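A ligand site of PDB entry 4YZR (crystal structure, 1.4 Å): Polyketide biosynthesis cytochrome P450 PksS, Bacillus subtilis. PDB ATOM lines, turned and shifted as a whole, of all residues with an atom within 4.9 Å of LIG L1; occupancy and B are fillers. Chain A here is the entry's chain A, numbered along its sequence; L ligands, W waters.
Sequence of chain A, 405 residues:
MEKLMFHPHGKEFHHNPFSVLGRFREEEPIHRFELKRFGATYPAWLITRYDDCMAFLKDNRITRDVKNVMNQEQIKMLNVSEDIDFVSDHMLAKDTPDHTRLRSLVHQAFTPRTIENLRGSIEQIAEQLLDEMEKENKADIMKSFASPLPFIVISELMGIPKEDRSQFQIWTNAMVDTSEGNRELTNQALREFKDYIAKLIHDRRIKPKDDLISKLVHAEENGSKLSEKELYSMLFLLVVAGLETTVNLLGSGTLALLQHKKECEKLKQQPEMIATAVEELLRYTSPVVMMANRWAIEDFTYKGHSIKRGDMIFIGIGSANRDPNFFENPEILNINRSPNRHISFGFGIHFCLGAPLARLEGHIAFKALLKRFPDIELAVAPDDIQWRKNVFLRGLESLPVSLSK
The backbone NH of Arg 103 is in hydrogen-bond range of the side-chain sulfur of Met 91 (3.7 Å).
O of Phe 345 sits at hydrogen-bond distance from N of Cys 352.
The backbone carbonyl oxygen (O) of Ala 241 lies within hydrogen-bond range of the side-chain hydroxyl (OG1) of Thr 245.
The backbone carbonyl oxygen (O) of Ala 241 sits at hydrogen-bond distance from the side-chain hydroxyl (OG1) of Thr 246 (3.1 Å).
The side-chain sulfur (SG) of Cys 352 sits close to the backbone NH (N) of Gly 354 (3.3 Å).
NH1 of Arg 103 is in hydrogen-bond range of O of Phe 351, at 2.7 Å.
O of Leu 282 sits at hydrogen-bond distance from OG of Ser 344 (2.7 Å).
The guanidinium group (NH2) of Arg 294 sits at hydrogen-bond distance from the backbone carbonyl oxygen (O) of Ala 292.
SD of Met 291 lies close to O1 of LIG L1 (3.5 Å).
CE of Met 91 touches O4 of LIG L1 (2.9 Å).
CA of Leu 92 touches O3 of LIG L1, 3.5 Å away.
Leu 237 touches LIG L1 (CD2 to C31, 3.7 Å).
O of Leu 238 touches C26 of LIG L1, at 3.5 Å.
Ala 241 touches LIG L1 (CB to C23, 3.1 Å).
CA of Gly 242 touches C24 of LIG L1 (3.8 Å).
Thr 245 touches LIG L1 (O to C19, 3.9 Å).
Thr 246 touches LIG L1.
Leu 249 touches LIG L1 (CB to C19, 3.7 Å).
Val 288 touches LIG L1.
Ser 344 touches LIG L1.
Phe 345 touches LIG L1.
N of Gly 346 touches C9 of LIG L1 (3.6 Å).
Ile 349 touches LIG L1 (O to O4, 3.7 Å).
Leu 353 touches LIG L1.
Gly 354 touches LIG L1.
CB of Ala 358 touches C18 of LIG L1, at 3.6 Å.
Hydrophobic or aromatic side chains that line LIG L1: Met 91, Leu 92, His 99, Leu 237, Leu 238, Ala 241, Leu 249, Val 288, Met 291, Phe 345, His 350, Leu 353 and Ala 358.
The nearest printed residue that does not touch LIG L1 is Phe 110 (4.02 Å).
The guanidinium group (NH2) of Arg 64 is in salt-bridge range of an oxygen (O1) of LIG L1, 2.8 Å away.
The guanidinium group (NH1) of Arg 294 is in salt-bridge range of an oxygen (O2) of LIG L1, at 2.9 Å.
A ring nitrogen (NE2) of His 99 sits at hydrogen-bond distance from an oxygen (O4) of LIG L1.
FE1 of LIG L1 is bound by SG of Cys 352 (2.3 Å).
O3 of LIG L1 lies within hydrogen-bond range of ND1 of His 350 (2.7 Å).
NH1 of Arg 103 lies within salt-bridge range of O4 of LIG L1, at 2.7 Å.
A nitrogen (N2) of LG2 L2 is bound to an iron atom (FE1) of LIG L1 (2.2 Å).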
ATOM      1  N   ARG A  64     -22.371 -13.100 -11.953  1.00  0.00           N
ATOM      2  CA  ARG A  64     -22.759 -11.738 -12.121  1.00  0.00           C
ATOM      3  C   ARG A  64     -24.082 -11.471 -11.451  1.00  0.00           C
ATOM      4  O   ARG A  64     -24.511 -10.401 -11.426  1.00  0.00           O
ATOM      5  CB  ARG A  64     -22.902 -11.407 -13.608  1.00  0.00           C
ATOM      6  CG  ARG A  64     -21.646 -11.590 -14.412  1.00  0.00           C
ATOM      7  CD  ARG A  64     -20.421 -10.963 -13.749  1.00  0.00           C
ATOM      8  NE  ARG A  64     -20.550  -9.527 -13.651  1.00  0.00           N
ATOM      9  CZ  ARG A  64     -20.310  -8.675 -14.642  1.00  0.00           C
ATOM     10  NH1 ARG A  64     -19.785  -9.090 -15.755  1.00  0.00           N
ATOM     11  NH2 ARG A  64     -20.536  -7.410 -14.444  1.00  0.00           N
ATOM     12  N   MET A  91     -29.071  -7.616 -18.444  1.00  0.00           N
ATOM     13  CA  MET A  91     -28.289  -8.754 -18.811  1.00  0.00           C
ATOM     14  C   MET A  91     -26.910  -8.782 -18.248  1.00  0.00           C
ATOM     15  O   MET A  91     -26.286  -9.862 -18.257  1.00  0.00           O
ATOM     16  CB  MET A  91     -28.242  -8.956 -20.313  1.00  0.00           C
ATOM     17  CG  MET A  91     -27.541  -7.971 -21.082  1.00  0.00           C
ATOM     18  SD  MET A  91     -27.884  -8.462 -22.835  1.00  0.00           S
ATOM     19  CE  MET A  91     -26.349  -8.874 -23.416  1.00  0.00           C
ATOM     20  N   LEU A  92     -26.337  -7.633 -17.889  1.00  0.00           N
ATOM     21  CA  LEU A  92     -25.023  -7.624 -17.354  1.00  0.00           C
ATOM     22  C   LEU A  92     -25.023  -8.168 -15.903  1.00  0.00           C
ATOM     23  O   LEU A  92     -23.977  -8.497 -15.351  1.00  0.00           O
ATOM     24  CB  LEU A  92     -24.508  -6.180 -17.549  1.00  0.00           C
ATOM     25  CG  LEU A  92     -23.077  -5.966 -17.104  1.00  0.00           C
ATOM     26  CD1 LEU A  92     -21.997  -6.838 -17.747  1.00  0.00           C
ATOM     27  CD2 LEU A  92     -22.695  -4.468 -17.411  1.00  0.00           C
ATOM     28  N   HIS A  99     -28.649 -15.037 -19.712  1.00  0.00           N
ATOM     29  CA  HIS A  99     -27.900 -13.988 -20.439  1.00  0.00           C
ATOM     30  C   HIS A  99     -27.947 -14.263 -21.911  1.00  0.00           C
ATOM     31  O   HIS A  99     -28.092 -13.294 -22.732  1.00  0.00           O
ATOM     32  CB  HIS A  99     -26.494 -13.995 -19.960  1.00  0.00           C
ATOM     33  CG  HIS A  99     -25.618 -13.125 -20.821  1.00  0.00           C
ATOM     34  ND1 HIS A  99     -24.928 -13.629 -21.859  1.00  0.00           N
ATOM     35  CD2 HIS A  99     -25.395 -11.774 -20.811  1.00  0.00           C
ATOM     36  CE1 HIS A  99     -24.280 -12.637 -22.485  1.00  0.00           C
ATOM     37  NE2 HIS A  99     -24.583 -11.525 -21.855  1.00  0.00           N
ATOM     38  N   ARG A 103     -29.127 -11.465 -24.702  1.00  0.00           N
ATOM     39  CA  ARG A 103     -28.151 -10.939 -25.653  1.00  0.00           C
ATOM     40  C   ARG A 103     -28.641 -11.199 -27.040  1.00  0.00           C
ATOM     41  O   ARG A 103     -28.469 -10.325 -27.908  1.00  0.00           O
ATOM     42  CB  ARG A 103     -26.786 -11.465 -25.395  1.00  0.00           C
ATOM     43  CG  ARG A 103     -25.777 -10.688 -26.240  1.00  0.00           C
ATOM     44  CD  ARG A 103     -24.510 -10.395 -25.647  1.00  0.00           C
ATOM     45  NE  ARG A 103     -23.605  -9.725 -26.595  1.00  0.00           N
ATOM     46  CZ  ARG A 103     -22.499  -9.092 -26.207  1.00  0.00           C
ATOM     47  NH1 ARG A 103     -22.289  -8.892 -24.950  1.00  0.00           N
ATOM     48  NH2 ARG A 103     -21.688  -8.659 -27.138  1.00  0.00           N
ATOM     49  N   PHE A 110     -26.751  -4.201 -32.902  1.00  0.00           N
ATOM     50  CA  PHE A 110     -25.347  -3.759 -32.813  1.00  0.00           C
ATOM     51  C   PHE A 110     -24.453  -4.552 -33.724  1.00  0.00           C
ATOM     52  O   PHE A 110     -23.237  -4.512 -33.527  1.00  0.00           O
ATOM     53  CB  PHE A 110     -24.937  -3.800 -31.319  1.00  0.00           C
ATOM     54  CG  PHE A 110     -25.594  -2.729 -30.495  1.00  0.00           C
ATOM     55  CD1 PHE A 110     -25.019  -1.475 -30.364  1.00  0.00           C
ATOM     56  CD2 PHE A 110     -26.752  -2.946 -29.873  1.00  0.00           C
ATOM     57  CE1 PHE A 110     -25.671  -0.493 -29.701  1.00  0.00           C
ATOM     58  CE2 PHE A 110     -27.504  -2.000 -29.179  1.00  0.00           C
ATOM     59  CZ  PHE A 110     -26.920  -0.737 -29.052  1.00  0.00           C
ATOM     60  N   ILE A 154     -27.277   8.776 -28.946  1.00  0.00           N
ATOM     61  CA  ILE A 154     -28.222   7.926 -28.213  1.00  0.00           C
ATOM     62  C   ILE A 154     -29.619   8.400 -28.401  1.00  0.00           C
ATOM     63  O   ILE A 154     -30.549   7.559 -28.545  1.00  0.00           O
ATOM     64  CB  ILE A 154     -27.901   7.831 -26.680  1.00  0.00           C
ATOM     65  CG1 ILE A 154     -26.905   6.832 -26.474  1.00  0.00           C
ATOM     66  CG2 ILE A 154     -29.170   7.566 -25.785  1.00  0.00           C
ATOM     67  CD1 ILE A 154     -27.455   5.420 -26.720  1.00  0.00           C
ATOM     68  N   LEU A 237     -29.923  -0.126 -19.506  1.00  0.00           N
ATOM     69  CA  LEU A 237     -28.514  -0.464 -19.643  1.00  0.00           C
ATOM     70  C   LEU A 237     -27.880   0.223 -20.856  1.00  0.00           C
ATOM     71  O   LEU A 237     -26.812   0.778 -20.844  1.00  0.00           O
ATOM     72  CB  LEU A 237     -28.373  -1.989 -19.763  1.00  0.00           C
ATOM     73  CG  LEU A 237     -26.905  -2.451 -19.956  1.00  0.00           C
ATOM     74  CD1 LEU A 237     -25.958  -1.943 -18.879  1.00  0.00           C
ATOM     75  CD2 LEU A 237     -27.111  -3.984 -20.082  1.00  0.00           C
ATOM     76  N   LEU A 238     -28.612   0.189 -22.002  1.00  0.00           N
ATOM     77  CA  LEU A 238     -28.082   0.778 -23.223  1.00  0.00           C
ATOM     78  C   LEU A 238     -27.872   2.302 -23.133  1.00  0.00           C
ATOM     79  O   LEU A 238     -26.903   2.893 -23.570  1.00  0.00           O
ATOM     80  CB  LEU A 238     -28.976   0.480 -24.398  1.00  0.00           C
ATOM     81  CG  LEU A 238     -29.043  -0.987 -24.813  1.00  0.00           C
ATOM     82  CD1 LEU A 238     -30.154  -1.251 -25.796  1.00  0.00           C
ATOM     83  CD2 LEU A 238     -27.741  -1.520 -25.375  1.00  0.00           C
ATOM     84  N   ALA A 241     -24.926   3.183 -20.843  1.00  0.00           N
ATOM     85  CA  ALA A 241     -23.625   2.885 -21.636  1.00  0.00           C
ATOM     86  C   ALA A 241     -23.299   3.861 -22.648  1.00  0.00           C
ATOM     87  O   ALA A 241     -22.133   4.366 -22.760  1.00  0.00           O
ATOM     88  CB  ALA A 241     -23.673   1.502 -22.146  1.00  0.00           C
ATOM     89  N   GLY A 242     -24.284   4.281 -23.380  1.00  0.00           N
ATOM     90  CA  GLY A 242     -24.127   5.224 -24.428  1.00  0.00           C
ATOM     91  C   GLY A 242     -23.799   6.623 -24.068  1.00  0.00           C
ATOM     92  O   GLY A 242     -23.451   7.480 -24.907  1.00  0.00           O
ATOM     93  N   THR A 245     -19.814   6.667 -20.239  1.00  0.00           N
ATOM     94  CA  THR A 245     -18.607   5.957 -20.544  1.00  0.00           C
ATOM     95  C   THR A 245     -18.086   6.282 -21.971  1.00  0.00           C
ATOM     96  O   THR A 245     -16.890   6.503 -22.204  1.00  0.00           O
ATOM     97  CB  THR A 245     -18.753   4.476 -20.185  1.00  0.00           C
ATOM     98  OG1 THR A 245     -19.930   3.944 -20.826  1.00  0.00           O
ATOM     99  CG2 THR A 245     -18.789   4.369 -18.788  1.00  0.00           C
ATOM    100  N   THR A 246     -19.023   6.472 -22.920  1.00  0.00           N
ATOM    101  CA  THR A 246     -18.628   6.891 -24.269  1.00  0.00           C
ATOM    102  C   THR A 246     -18.132   8.333 -24.266  1.00  0.00           C
ATOM    103  O   THR A 246     -17.153   8.636 -24.901  1.00  0.00           O
ATOM    104  CB  THR A 246     -19.904   6.740 -25.169  1.00  0.00           C
ATOM    105  OG1 THR A 246     -20.357   5.342 -25.116  1.00  0.00           O
ATOM    106  CG2 THR A 246     -19.587   7.001 -26.520  1.00  0.00           C
ATOM    107  N   LEU A 249     -14.569   8.139 -23.212  1.00  0.00           N
ATOM    108  CA  LEU A 249     -13.634   7.844 -24.296  1.00  0.00           C
ATOM    109  C   LEU A 249     -13.258   9.139 -25.021  1.00  0.00           C
ATOM    110  O   LEU A 249     -12.097   9.415 -25.345  1.00  0.00           O
ATOM    111  CB  LEU A 249     -14.181   6.818 -25.277  1.00  0.00           C
ATOM    112  CG  LEU A 249     -13.358   6.560 -26.541  1.00  0.00           C
ATOM    113  CD1 LEU A 249     -11.919   6.098 -26.255  1.00  0.00           C
ATOM    114  CD2 LEU A 249     -14.020   5.570 -27.465  1.00  0.00           C
ATOM    115  N   LEU A 282      -8.423   3.598 -26.198  1.00  0.00           N
ATOM    116  CA  LEU A 282      -9.160   2.714 -25.285  1.00  0.00           C
ATOM    117  C   LEU A 282      -8.251   2.063 -24.313  1.00  0.00           C
ATOM    118  O   LEU A 282      -8.556   2.015 -23.095  1.00  0.00           O
ATOM    119  CB  LEU A 282      -9.900   1.675 -26.085  1.00  0.00           C
ATOM    120  CG  LEU A 282     -11.175   2.117 -26.768  1.00  0.00           C
ATOM    121  CD1 LEU A 282     -11.573   1.296 -27.964  1.00  0.00           C
ATOM    122  CD2 LEU A 282     -12.331   2.204 -25.732  1.00  0.00           C
ATOM    123  N   PRO A 287     -11.698   3.950 -20.057  1.00  0.00           N
ATOM    124  CA  PRO A 287     -12.848   4.709 -19.530  1.00  0.00           C
ATOM    125  C   PRO A 287     -13.501   3.978 -18.422  1.00  0.00           C
ATOM    126  O   PRO A 287     -13.942   4.593 -17.412  1.00  0.00           O
ATOM    127  CB  PRO A 287     -13.710   4.907 -20.735  1.00  0.00           C
ATOM    128  CG  PRO A 287     -12.744   4.903 -21.913  1.00  0.00           C
ATOM    129  CD  PRO A 287     -11.685   3.889 -21.555  1.00  0.00           C
ATOM    130  N   VAL A 288     -13.707   2.682 -18.550  1.00  0.00           N
ATOM    131  CA  VAL A 288     -14.023   1.814 -17.421  1.00  0.00           C
ATOM    132  C   VAL A 288     -12.693   1.352 -16.887  1.00  0.00           C
ATOM    133  O   VAL A 288     -11.991   0.478 -17.464  1.00  0.00           O
ATOM    134  CB  VAL A 288     -14.920   0.655 -17.813  1.00  0.00           C
ATOM    135  CG1 VAL A 288     -15.198  -0.178 -16.588  1.00  0.00           C
ATOM    136  CG2 VAL A 288     -16.172   1.136 -18.495  1.00  0.00           C
ATOM    137  N   MET A 291     -13.782  -2.854 -13.019  1.00  0.00           N
ATOM    138  CA  MET A 291     -15.192  -3.340 -12.980  1.00  0.00           C
ATOM    139  C   MET A 291     -15.373  -4.382 -11.937  1.00  0.00           C
ATOM    140  O   MET A 291     -14.390  -5.147 -11.669  1.00  0.00           O
ATOM    141  CB  MET A 291     -15.638  -3.804 -14.360  1.00  0.00           C
ATOM    142  CG  MET A 291     -14.827  -4.807 -14.989  1.00  0.00           C
ATOM    143  SD  MET A 291     -15.391  -5.279 -16.650  1.00  0.00           S
ATOM    144  CE  MET A 291     -14.156  -6.394 -17.083  1.00  0.00           C
ATOM    145  N   ALA A 292     -16.533  -4.450 -11.365  1.00  0.00           N
ATOM    146  CA  ALA A 292     -16.782  -5.418 -10.312  1.00  0.00           C
ATOM    147  C   ALA A 292     -18.105  -6.087 -10.561  1.00  0.00           C
ATOM    148  O   ALA A 292     -18.294  -6.633 -11.571  1.00  0.00           O
ATOM    149  CB  ALA A 292     -16.705  -4.734  -8.941  1.00  0.00           C
ATOM    150  N   ARG A 294     -19.176  -8.793  -9.495  1.00  0.00           N
ATOM    151  CA  ARG A 294     -18.716 -10.158  -9.714  1.00  0.00           C
ATOM    152  C   ARG A 294     -18.550 -10.798  -8.327  1.00  0.00           C
ATOM    153  O   ARG A 294     -17.949 -10.149  -7.499  1.00  0.00           O
ATOM    154  CB  ARG A 294     -17.362 -10.227 -10.415  1.00  0.00           C
ATOM    155  CG  ARG A 294     -17.492  -9.959 -11.856  1.00  0.00           C
ATOM    156  CD  ARG A 294     -16.162  -9.442 -12.385  1.00  0.00           C
ATOM    157  NE  ARG A 294     -16.127  -9.495 -13.861  1.00  0.00           N
ATOM    158  CZ  ARG A 294     -16.595  -8.508 -14.668  1.00  0.00           C
ATOM    159  NH1 ARG A 294     -16.562  -8.767 -15.948  1.00  0.00           N
ATOM    160  NH2 ARG A 294     -17.065  -7.438 -14.146  1.00  0.00           N
ATOM    161  N   ILE A 317      -8.981  -3.313 -15.003  1.00  0.00           N
ATOM    162  CA  ILE A 317      -8.758  -3.017 -16.428  1.00  0.00           C
ATOM    163  C   ILE A 317      -7.592  -2.105 -16.663  1.00  0.00           C
ATOM    164  O   ILE A 317      -6.746  -2.345 -17.538  1.00  0.00           O
ATOM    165  CB  ILE A 317     -10.061  -2.460 -17.060  1.00  0.00           C
ATOM    166  CG1 ILE A 317     -11.151  -3.480 -17.095  1.00  0.00           C
ATOM    167  CG2 ILE A 317      -9.805  -1.966 -18.458  1.00  0.00           C
ATOM    168  CD1 ILE A 317     -12.517  -2.997 -17.632  1.00  0.00           C
ATOM    169  N   SER A 344     -10.461  -3.154 -22.463  1.00  0.00           N
ATOM    170  CA  SER A 344     -11.320  -1.992 -22.157  1.00  0.00           C
ATOM    171  C   SER A 344     -12.794  -2.194 -22.350  1.00  0.00           C
ATOM    172  O   SER A 344     -13.601  -1.480 -21.762  1.00  0.00           O
ATOM    173  CB  SER A 344     -10.923  -0.807 -22.887  1.00  0.00           C
ATOM    174  OG  SER A 344      -9.500  -0.506 -22.568  1.00  0.00           O
ATOM    175  N   PHE A 345     -13.140  -3.157 -23.190  1.00  0.00           N
ATOM    176  CA  PHE A 345     -14.562  -3.593 -23.476  1.00  0.00           C
ATOM    177  C   PHE A 345     -14.896  -4.874 -22.698  1.00  0.00           C
ATOM    178  O   PHE A 345     -15.892  -5.527 -22.966  1.00  0.00           O
ATOM    179  CB  PHE A 345     -14.806  -3.743 -24.927  1.00  0.00           C
ATOM    180  CG  PHE A 345     -14.796  -2.473 -25.717  1.00  0.00           C
ATOM    181  CD1 PHE A 345     -15.647  -1.420 -25.420  1.00  0.00           C
ATOM    182  CD2 PHE A 345     -14.006  -2.315 -26.885  1.00  0.00           C
ATOM    183  CE1 PHE A 345     -15.718  -0.274 -26.130  1.00  0.00           C
ATOM    184  CE2 PHE A 345     -14.075  -1.192 -27.649  1.00  0.00           C
ATOM    185  CZ  PHE A 345     -14.930  -0.175 -27.301  1.00  0.00           C
ATOM    186  N   GLY A 346     -14.008  -5.279 -21.754  1.00  0.00           N
ATOM    187  CA  GLY A 346     -14.168  -6.529 -21.052  1.00  0.00           C
ATOM    188  C   GLY A 346     -13.717  -7.658 -21.935  1.00  0.00           C
ATOM    189  O   GLY A 346     -12.853  -7.525 -22.805  1.00  0.00           O
ATOM    190  N   ILE A 349     -18.208 -13.477 -22.125  1.00  0.00           N
ATOM    191  CA  ILE A 349     -19.642 -13.510 -22.199  1.00  0.00           C
ATOM    192  C   ILE A 349     -20.278 -12.110 -22.308  1.00  0.00           C
ATOM    193  O   ILE A 349     -21.197 -11.865 -23.103  1.00  0.00           O
ATOM    194  CB  ILE A 349     -20.220 -14.331 -20.921  1.00  0.00           C
ATOM    195  CG1 ILE A 349     -19.844 -15.823 -21.028  1.00  0.00           C
ATOM    196  CG2 ILE A 349     -21.684 -14.246 -20.773  1.00  0.00           C
ATOM    197  CD1 ILE A 349     -20.071 -16.663 -19.732  1.00  0.00           C
ATOM    198  N   HIS A 350     -19.747 -11.239 -21.501  1.00  0.00           N
ATOM    199  CA  HIS A 350     -20.298  -9.900 -21.279  1.00  0.00           C
ATOM    200  C   HIS A 350     -19.474  -8.839 -22.077  1.00  0.00           C
ATOM    201  O   HIS A 350     -19.706  -7.645 -21.775  1.00  0.00           O
ATOM    202  CB  HIS A 350     -20.410  -9.572 -19.883  1.00  0.00           C
ATOM    203  CG  HIS A 350     -21.347 -10.473 -19.112  1.00  0.00           C
ATOM    204  ND1 HIS A 350     -22.692 -10.280 -19.117  1.00  0.00           N
ATOM    205  CD2 HIS A 350     -21.112 -11.578 -18.352  1.00  0.00           C
ATOM    206  CE1 HIS A 350     -23.284 -11.220 -18.337  1.00  0.00           C
ATOM    207  NE2 HIS A 350     -22.349 -11.989 -17.895  1.00  0.00           N
ATOM    208  N   PHE A 351     -18.693  -9.234 -23.039  1.00  0.00           N
ATOM    209  CA  PHE A 351     -17.937  -8.263 -23.818  1.00  0.00           C
ATOM    210  C   PHE A 351     -18.920  -7.202 -24.335  1.00  0.00           C
ATOM    211  O   PHE A 351     -19.998  -7.482 -24.917  1.00  0.00           O
ATOM    212  CB  PHE A 351     -17.287  -8.979 -25.005  1.00  0.00           C
ATOM    213  CG  PHE A 351     -16.507  -8.092 -25.915  1.00  0.00           C
ATOM    214  CD1 PHE A 351     -15.186  -7.811 -25.649  1.00  0.00           C
ATOM    215  CD2 PHE A 351     -17.083  -7.447 -26.948  1.00  0.00           C
ATOM    216  CE1 PHE A 351     -14.493  -6.951 -26.451  1.00  0.00           C
ATOM    217  CE2 PHE A 351     -16.403  -6.558 -27.731  1.00  0.00           C
ATOM    218  CZ  PHE A 351     -15.083  -6.317 -27.516  1.00  0.00           C
ATOM    219  N   CYS A 352     -18.464  -5.939 -24.296  1.00  0.00           N
ATOM    220  CA  CYS A 352     -19.363  -4.842 -24.633  1.00  0.00           C
ATOM    221  C   CYS A 352     -20.087  -4.993 -25.906  1.00  0.00           C
ATOM    222  O   CYS A 352     -19.569  -5.033 -26.965  1.00  0.00           O
ATOM    223  CB  CYS A 352     -18.487  -3.591 -24.675  1.00  0.00           C
ATOM    224  SG  CYS A 352     -19.426  -2.077 -25.054  1.00  0.00           S
ATOM    225  N   LEU A 353     -21.407  -4.913 -25.791  1.00  0.00           N
ATOM    226  CA  LEU A 353     -22.319  -4.921 -26.929  1.00  0.00           C
ATOM    227  C   LEU A 353     -22.186  -3.719 -27.808  1.00  0.00           C
ATOM    228  O   LEU A 353     -22.345  -3.763 -29.004  1.00  0.00           O
ATOM    229  CB  LEU A 353     -23.731  -5.053 -26.412  1.00  0.00           C
ATOM    230  CG  LEU A 353     -24.865  -5.114 -27.488  1.00  0.00           C
ATOM    231  CD1 LEU A 353     -24.834  -6.460 -28.171  1.00  0.00           C
ATOM    232  CD2 LEU A 353     -26.166  -4.794 -26.811  1.00  0.00           C
ATOM    233  N   GLY A 354     -21.909  -2.612 -27.179  1.00  0.00           N
ATOM    234  CA  GLY A 354     -21.828  -1.314 -27.887  1.00  0.00           C
ATOM    235  C   GLY A 354     -20.501  -1.005 -28.471  1.00  0.00           C
ATOM    236  O   GLY A 354     -20.318   0.084 -29.029  1.00  0.00           O
ATOM    237  N   LEU A 357     -20.235   0.823 -31.779  1.00  0.00           N
ATOM    238  CA  LEU A 357     -20.740   2.194 -31.744  1.00  0.00           C
ATOM    239  C   LEU A 357     -19.767   3.093 -31.038  1.00  0.00           C
ATOM    240  O   LEU A 357     -19.486   4.180 -31.507  1.00  0.00           O
ATOM    241  CB  LEU A 357     -22.118   2.236 -31.039  1.00  0.00           C
ATOM    242  CG  LEU A 357     -22.702   3.634 -30.917  1.00  0.00           C
ATOM    243  CD1 LEU A 357     -22.889   4.280 -32.285  1.00  0.00           C
ATOM    244  CD2 LEU A 357     -24.101   3.450 -30.281  1.00  0.00           C
ATOM    245  N   ALA A 358     -19.196   2.657 -29.918  1.00  0.00           N
ATOM    246  CA  ALA A 358     -18.148   3.448 -29.267  1.00  0.00           C
ATOM    247  C   ALA A 358     -16.997   3.689 -30.188  1.00  0.00           C
ATOM    248  O   ALA A 358     -16.457   4.802 -30.310  1.00  0.00           O
ATOM    249  CB  ALA A 358     -17.717   2.722 -28.044  1.00  0.00           C
HETATM  250  C1  LIG L   1     -20.596  -4.158 -21.360  1.00  0.00           C
HETATM  251  C2  LIG L   1     -17.047  -0.897 -21.737  1.00  0.00           C
HETATM  252  C3  LIG L   1     -19.862   1.801 -24.652  1.00  0.00           C
HETATM  253  C4  LIG L   1     -23.407  -1.390 -24.119  1.00  0.00           C
HETATM  254  C5  LIG L   1     -19.406  -3.509 -21.188  1.00  0.00           C
HETATM  255  C6  LIG L   1     -18.220  -3.963 -20.437  1.00  0.00           C
HETATM  256  C7  LIG L   1     -17.302  -3.036 -20.500  1.00  0.00           C
HETATM  257  C8  LIG L   1     -17.797  -1.985 -21.380  1.00  0.00           C
HETATM  258  C9  LIG L   1     -16.002  -3.008 -19.803  1.00  0.00           C
HETATM  259  C10 LIG L   1     -18.182  -5.243 -19.591  1.00  0.00           C
HETATM  260  C11 LIG L   1     -18.606  -5.017 -18.206  1.00  0.00           C
HETATM  261  C12 LIG L   1     -18.555  -6.247 -17.209  1.00  0.00           C
HETATM  262  O1  LIG L   1     -18.787  -5.905 -15.995  1.00  0.00           O
HETATM  263  O2  LIG L   1     -18.273  -7.271 -17.718  1.00  0.00           O
HETATM  264  C13 LIG L   1     -17.509   0.127 -22.561  1.00  0.00           C
HETATM  265  C14 LIG L   1     -16.754   1.256 -23.001  1.00  0.00           C
HETATM  266  C15 LIG L   1     -17.504   2.040 -23.807  1.00  0.00           C
HETATM  267  C16 LIG L   1     -18.798   1.362 -23.890  1.00  0.00           C
HETATM  268  C17 LIG L   1     -15.365   1.456 -22.588  1.00  0.00           C
HETATM  269  C18 LIG L   1     -17.226   3.284 -24.506  1.00  0.00           C
HETATM  270  C19 LIG L   1     -16.022   3.663 -24.750  1.00  0.00           C
HETATM  271  C20 LIG L   1     -21.073   1.190 -24.827  1.00  0.00           C
HETATM  272  C21 LIG L   1     -22.175   1.633 -25.587  1.00  0.00           C
HETATM  273  C22 LIG L   1     -23.216   0.714 -25.439  1.00  0.00           C
HETATM  274  C23 LIG L   1     -22.720  -0.279 -24.533  1.00  0.00           C
HETATM  275  C24 LIG L   1     -22.073   2.818 -26.507  1.00  0.00           C
HETATM  276  C25 LIG L   1     -24.539   0.715 -26.040  1.00  0.00           C
HETATM  277  C26 LIG L   1     -25.158   1.793 -26.394  1.00  0.00           C
HETATM  278  C27 LIG L   1     -22.992  -2.420 -23.314  1.00  0.00           C
HETATM  279  C28 LIG L   1     -23.820  -3.522 -22.898  1.00  0.00           C
HETATM  280  C29 LIG L   1     -23.013  -4.315 -22.134  1.00  0.00           C
HETATM  281  C30 LIG L   1     -21.669  -3.699 -22.094  1.00  0.00           C
HETATM  282  C31 LIG L   1     -25.253  -3.786 -23.296  1.00  0.00           C
HETATM  283  C32 LIG L   1     -23.361  -5.620 -21.473  1.00  0.00           C
HETATM  284  C33 LIG L   1     -23.093  -6.800 -22.347  1.00  0.00           C
HETATM  285  C34 LIG L   1     -23.532  -8.183 -21.783  1.00  0.00           C
HETATM  286  O3  LIG L   1     -23.726  -8.229 -20.561  1.00  0.00           O
HETATM  287  O4  LIG L   1     -23.579  -9.117 -22.603  1.00  0.00           O
HETATM  288  N1  LIG L   1     -19.040  -2.350 -21.802  1.00  0.00           N
HETATM  289  N2  LIG L   1     -18.746   0.208 -23.168  1.00  0.00           N
HETATM  290  N3  LIG L   1     -21.419   0.024 -24.208  1.00  0.00           N
HETATM  291  N4  LIG L   1     -21.718  -2.512 -22.824  1.00  0.00           N
HETATM  292 FE1  LIG L   1     -20.215  -1.204 -23.052  1.00  0.00          FE
HETATM  293  C1  LG2 L   2     -21.084   1.001 -19.525  1.00  0.00           C
HETATM  294  N1  LG2 L   2     -21.966  -0.073 -19.354  1.00  0.00           N
HETATM  295  C2  LG2 L   2     -20.484   0.806 -20.714  1.00  0.00           C
HETATM  296  C3  LG2 L   2     -21.842  -0.882 -20.393  1.00  0.00           C
HETATM  297  N2  LG2 L   2     -20.948  -0.334 -21.226  1.00  0.00           N
HETATM  298  O   HOH W   1     -19.707  -3.694 -14.778  1.00  0.00           O
HETATM  299  O   HOH W   2     -16.541  -8.542 -19.641  1.00  0.00           O
